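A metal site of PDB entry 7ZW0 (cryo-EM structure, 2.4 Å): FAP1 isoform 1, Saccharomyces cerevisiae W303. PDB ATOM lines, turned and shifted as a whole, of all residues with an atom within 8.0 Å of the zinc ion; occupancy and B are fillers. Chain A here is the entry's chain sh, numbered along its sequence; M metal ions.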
ATOM      1  N   LEU A 583      -4.629   2.573  10.032  1.00  0.00           N
ATOM      2  CA  LEU A 583      -4.100   1.299   9.572  1.00  0.00           C
ATOM      3  C   LEU A 583      -3.002   0.819  10.501  1.00  0.00           C
ATOM      4  O   LEU A 583      -2.267   1.623  11.066  1.00  0.00           O
ATOM      5  CB  LEU A 583      -3.617   1.464   8.138  1.00  0.00           C
ATOM      6  CG  LEU A 583      -4.791   1.900   7.255  1.00  0.00           C
ATOM      7  CD1 LEU A 583      -4.377   2.672   6.025  1.00  0.00           C
ATOM      8  CD2 LEU A 583      -5.682   0.722   6.900  1.00  0.00           C
ATOM      9  N   TYR A 585      -0.333  -1.099   9.629  1.00  0.00           N
ATOM     10  CA  TYR A 585       0.957  -1.006   8.940  1.00  0.00           C
ATOM     11  C   TYR A 585       1.453   0.395   8.640  1.00  0.00           C
ATOM     12  O   TYR A 585       2.629   0.602   8.397  1.00  0.00           O
ATOM     13  CB  TYR A 585       0.871  -1.782   7.625  1.00  0.00           C
ATOM     14  CG  TYR A 585      -0.162  -1.216   6.672  1.00  0.00           C
ATOM     15  CD1 TYR A 585      -1.511  -1.530   6.822  1.00  0.00           C
ATOM     16  CD2 TYR A 585       0.198  -0.362   5.650  1.00  0.00           C
ATOM     17  CE1 TYR A 585      -2.462  -1.005   5.981  1.00  0.00           C
ATOM     18  CE2 TYR A 585      -0.748   0.171   4.806  1.00  0.00           C
ATOM     19  CZ  TYR A 585      -2.074  -0.154   4.970  1.00  0.00           C
ATOM     20  OH  TYR A 585      -3.018   0.365   4.126  1.00  0.00           O
ATOM     21  N   CYS A 586       0.542   1.353   8.648  1.00  0.00           N
ATOM     22  CA  CYS A 586       0.946   2.688   8.273  1.00  0.00           C
ATOM     23  C   CYS A 586       0.536   3.699   9.307  1.00  0.00           C
ATOM     24  O   CYS A 586      -0.376   3.460  10.087  1.00  0.00           O
ATOM     25  CB  CYS A 586       0.381   3.067   6.913  1.00  0.00           C
ATOM     26  SG  CYS A 586       1.655   3.136   5.638  1.00  0.00           S
ATOM     27  N   TYR A 587       1.218   4.833   9.329  1.00  0.00           N
ATOM     28  CA  TYR A 587       0.837   5.891  10.239  1.00  0.00           C
ATOM     29  C   TYR A 587      -0.565   6.310   9.881  1.00  0.00           C
ATOM     30  O   TYR A 587      -1.388   6.587  10.756  1.00  0.00           O
ATOM     31  CB  TYR A 587       1.762   7.082  10.027  1.00  0.00           C
ATOM     32  CG  TYR A 587       3.179   6.862  10.457  1.00  0.00           C
ATOM     33  CD1 TYR A 587       3.474   6.371  11.730  1.00  0.00           C
ATOM     34  CD2 TYR A 587       4.244   7.146   9.611  1.00  0.00           C
ATOM     35  CE1 TYR A 587       4.775   6.170  12.128  1.00  0.00           C
ATOM     36  CE2 TYR A 587       5.545   6.945  10.008  1.00  0.00           C
ATOM     37  CZ  TYR A 587       5.801   6.463  11.264  1.00  0.00           C
ATOM     38  OH  TYR A 587       7.101   6.255  11.674  1.00  0.00           O
ATOM     39  N   HIS A 588      -0.862   6.342   8.590  1.00  0.00           N
ATOM     40  CA  HIS A 588      -2.168   6.817   8.123  1.00  0.00           C
ATOM     41  C   HIS A 588      -3.396   5.929   8.317  1.00  0.00           C
ATOM     42  O   HIS A 588      -3.275   4.718   8.490  1.00  0.00           O
ATOM     43  CB  HIS A 588      -1.998   7.254   6.679  1.00  0.00           C
ATOM     44  CG  HIS A 588      -0.766   8.056   6.471  1.00  0.00           C
ATOM     45  ND1 HIS A 588       0.423   7.513   6.018  1.00  0.00           N
ATOM     46  CD2 HIS A 588      -0.498   9.361   6.728  1.00  0.00           C
ATOM     47  CE1 HIS A 588       1.346   8.447   5.974  1.00  0.00           C
ATOM     48  NE2 HIS A 588       0.809   9.582   6.398  1.00  0.00           N
ATOM     49  N   THR A 589      -4.596   6.502   8.230  1.00  0.00           N
ATOM     50  CA  THR A 589      -5.831   5.740   8.403  1.00  0.00           C
ATOM     51  C   THR A 589      -6.402   5.270   7.078  1.00  0.00           C
ATOM     52  O   THR A 589      -5.876   5.616   6.021  1.00  0.00           O
ATOM     53  CB  THR A 589      -6.916   6.601   9.063  1.00  0.00           C
ATOM     54  OG1 THR A 589      -7.477   7.492   8.093  1.00  0.00           O
ATOM     55  CG2 THR A 589      -6.345   7.390  10.215  1.00  0.00           C
ATOM     56  N   GLN A 601      -8.253  -0.907   3.952  1.00  0.00           N
ATOM     57  CA  GLN A 601      -7.249  -0.963   2.884  1.00  0.00           C
ATOM     58  C   GLN A 601      -5.916  -1.596   3.260  1.00  0.00           C
ATOM     59  O   GLN A 601      -5.415  -1.411   4.360  1.00  0.00           O
ATOM     60  CB  GLN A 601      -7.021   0.415   2.262  1.00  0.00           C
ATOM     61  CG  GLN A 601      -6.413   1.468   3.166  1.00  0.00           C
ATOM     62  CD  GLN A 601      -6.261   2.803   2.459  1.00  0.00           C
ATOM     63  OE1 GLN A 601      -6.579   2.931   1.275  1.00  0.00           O
ATOM     64  NE2 GLN A 601      -5.770   3.804   3.177  1.00  0.00           N
ATOM     65  N   VAL A 603      -2.987  -1.403   1.222  1.00  0.00           N
ATOM     66  CA  VAL A 603      -1.858  -0.539   0.951  1.00  0.00           C
ATOM     67  C   VAL A 603      -2.223   0.905   1.220  1.00  0.00           C
ATOM     68  O   VAL A 603      -3.354   1.316   1.014  1.00  0.00           O
ATOM     69  CB  VAL A 603      -1.358  -0.666  -0.502  1.00  0.00           C
ATOM     70  CG1 VAL A 603      -0.491  -1.909  -0.657  1.00  0.00           C
ATOM     71  CG2 VAL A 603      -2.529  -0.705  -1.468  1.00  0.00           C
ATOM     72  N   CYS A 604      -1.254   1.664   1.706  1.00  0.00           N
ATOM     73  CA  CYS A 604      -1.533   3.049   2.022  1.00  0.00           C
ATOM     74  C   CYS A 604      -0.904   3.887   0.959  1.00  0.00           C
ATOM     75  O   CYS A 604       0.280   3.736   0.673  1.00  0.00           O
ATOM     76  CB  CYS A 604      -0.955   3.401   3.388  1.00  0.00           C
ATOM     77  SG  CYS A 604      -1.159   5.133   3.866  1.00  0.00           S
ATOM     78  N   LYS A 605      -1.695   4.744   0.333  1.00  0.00           N
ATOM     79  CA  LYS A 605      -1.135   5.639  -0.676  1.00  0.00           C
ATOM     80  C   LYS A 605      -0.949   7.053  -0.159  1.00  0.00           C
ATOM     81  O   LYS A 605      -0.543   7.941  -0.911  1.00  0.00           O
ATOM     82  CB  LYS A 605      -1.982   5.615  -1.935  1.00  0.00           C
ATOM     83  CG  LYS A 605      -1.645   4.457  -2.850  1.00  0.00           C
ATOM     84  CD  LYS A 605      -0.176   4.483  -3.214  1.00  0.00           C
ATOM     85  CE  LYS A 605       0.195   3.364  -4.167  1.00  0.00           C
ATOM     86  NZ  LYS A 605       1.621   3.439  -4.584  1.00  0.00           N
ATOM     87  N   GLN A 606      -1.246   7.284   1.105  1.00  0.00           N
ATOM     88  CA  GLN A 606      -1.083   8.613   1.693  1.00  0.00           C
ATOM     89  C   GLN A 606       0.384   8.994   1.867  1.00  0.00           C
ATOM     90  O   GLN A 606       1.212   8.146   2.153  1.00  0.00           O
ATOM     91  CB  GLN A 606      -1.820   8.710   3.028  1.00  0.00           C
ATOM     92  CG  GLN A 606      -3.283   8.313   2.952  1.00  0.00           C
ATOM     93  CD  GLN A 606      -4.063   8.700   4.188  1.00  0.00           C
ATOM     94  OE1 GLN A 606      -5.057   8.064   4.532  1.00  0.00           O
ATOM     95  NE2 GLN A 606      -3.597   9.731   4.869  1.00  0.00           N
ATOM     96  N   THR A 607       0.704  10.270   1.684  1.00  0.00           N
ATOM     97  CA  THR A 607       2.078  10.725   1.876  1.00  0.00           C
ATOM     98  C   THR A 607       2.444  10.754   3.350  1.00  0.00           C
ATOM     99  O   THR A 607       1.567  10.965   4.188  1.00  0.00           O
ATOM    100  CB  THR A 607       2.291  12.123   1.279  1.00  0.00           C
ATOM    101  OG1 THR A 607       1.308  13.027   1.808  1.00  0.00           O
ATOM    102  CG2 THR A 607       2.165  12.074  -0.234  1.00  0.00           C
ATOM    103  N   CYS A 608       3.723  10.597   3.687  1.00  0.00           N
ATOM    104  CA  CYS A 608       4.128  10.506   5.092  1.00  0.00           C
ATOM    105  C   CYS A 608       3.813  11.728   5.948  1.00  0.00           C
ATOM    106  O   CYS A 608       3.372  11.576   7.093  1.00  0.00           O
ATOM    107  CB  CYS A 608       5.602  10.135   5.210  1.00  0.00           C
ATOM    108  SG  CYS A 608       6.012   9.244   6.728  1.00  0.00           S
ATOM    109  N   PRO A 622       6.462   9.687   0.497  1.00  0.00           N
ATOM    110  CA  PRO A 622       5.219   8.943   0.768  1.00  0.00           C
ATOM    111  C   PRO A 622       5.317   8.126   2.035  1.00  0.00           C
ATOM    112  O   PRO A 622       6.407   8.012   2.595  1.00  0.00           O
ATOM    113  CB  PRO A 622       5.088   8.009  -0.437  1.00  0.00           C
ATOM    114  CG  PRO A 622       6.467   7.885  -0.987  1.00  0.00           C
ATOM    115  CD  PRO A 622       7.095   9.229  -0.760  1.00  0.00           C
ATOM    116  N   CYS A 623       4.212   7.559   2.482  1.00  0.00           N
ATOM    117  CA  CYS A 623       4.232   6.883   3.766  1.00  0.00           C
ATOM    118  C   CYS A 623       5.350   5.858   3.867  1.00  0.00           C
ATOM    119  O   CYS A 623       5.555   5.048   2.970  1.00  0.00           O
ATOM    120  CB  CYS A 623       2.906   6.169   3.992  1.00  0.00           C
ATOM    121  SG  CYS A 623       2.402   5.113   2.614  1.00  0.00           S
ATOM    122  N   HIS A 624       6.074   5.908   4.968  1.00  0.00           N
ATOM    123  CA  HIS A 624       7.156   4.962   5.172  1.00  0.00           C
ATOM    124  C   HIS A 624       6.732   3.844   6.096  1.00  0.00           C
ATOM    125  O   HIS A 624       7.542   3.006   6.474  1.00  0.00           O
ATOM    126  CB  HIS A 624       8.385   5.679   5.699  1.00  0.00           C
ATOM    127  CG  HIS A 624       8.884   6.749   4.794  1.00  0.00           C
ATOM    128  ND1 HIS A 624       8.495   8.061   4.913  1.00  0.00           N
ATOM    129  CD2 HIS A 624       9.710   6.691   3.723  1.00  0.00           C
ATOM    130  CE1 HIS A 624       9.089   8.778   3.974  1.00  0.00           C
ATOM    131  NE2 HIS A 624       9.826   7.968   3.231  1.00  0.00           N
ATOM    132  N   GLY A 625       5.465   3.845   6.474  1.00  0.00           N
ATOM    133  CA  GLY A 625       4.958   2.785   7.326  1.00  0.00           C
ATOM    134  C   GLY A 625       5.462   2.951   8.742  1.00  0.00           C
ATOM    135  O   GLY A 625       5.822   4.040   9.146  1.00  0.00           O
ATOM    136  N   LYS A 626       5.479   1.862   9.496  1.00  0.00           N
ATOM    137  CA  LYS A 626       5.954   1.915  10.869  1.00  0.00           C
ATOM    138  C   LYS A 626       7.301   2.630  11.046  1.00  0.00           C
ATOM    139  O   LYS A 626       7.441   3.429  11.958  1.00  0.00           O
ATOM    140  CB  LYS A 626       6.005   0.500  11.448  1.00  0.00           C
ATOM    141  CG  LYS A 626       4.661  -0.209  11.389  1.00  0.00           C
ATOM    142  CD  LYS A 626       4.743  -1.621  11.934  1.00  0.00           C
ATOM    143  CE  LYS A 626       3.374  -2.289  11.901  1.00  0.00           C
ATOM    144  NZ  LYS A 626       3.403  -3.655  12.495  1.00  0.00           N
HETATM  145 ZN    ZN M   1       0.441   5.306   4.679  1.00  0.00          ZN
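The side-chain sulfur of Cys 623 is in hydrogen-bond range of the backbone carbonyl oxygen of Cys 604 (3.2 Å). The side-chain sulfur of Cys 604 lies close to the backbone NH of Gln 606 (3.5 Å). The backbone NH of Cys 604 is in hydrogen-bond range of the side-chain hydroxyl of Tyr 585, 3.3 Å away. The backbone carbonyl oxygen of His 588 is in hydrogen-bond range of the backbone NH of Leu 583, 3.0 Å away. NE2 of His 588 is in hydrogen-bond range of O of Thr 607, at 2.7 Å. A ring nitrogen (NE2) of His 588 lies within hydrogen-bond range of the backbone carbonyl oxygen of Cys 608 (3.3 Å). The backbone NH (N) of Cys 623 sits at hydrogen-bond distance from the backbone carbonyl oxygen (O) of Gln 606 (3.1 Å). The side-chain amide oxygen of Gln 606 sits close to the backbone carbonyl oxygen of Thr 589 (3.0 Å).
Gln 606 touches the zinc ion (O to ZN, 3.9 Å).
The zinc ion is bound by the side-chain sulfur (SG) of Cys 604, a ring nitrogen (ND1) of His 588 and the side-chain sulfur (SG) of Cys 586. The zinc ion has three donor atoms within binding distance. Slightly farther from the zinc ion lies SG of Cys 623 (2.9 Å).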
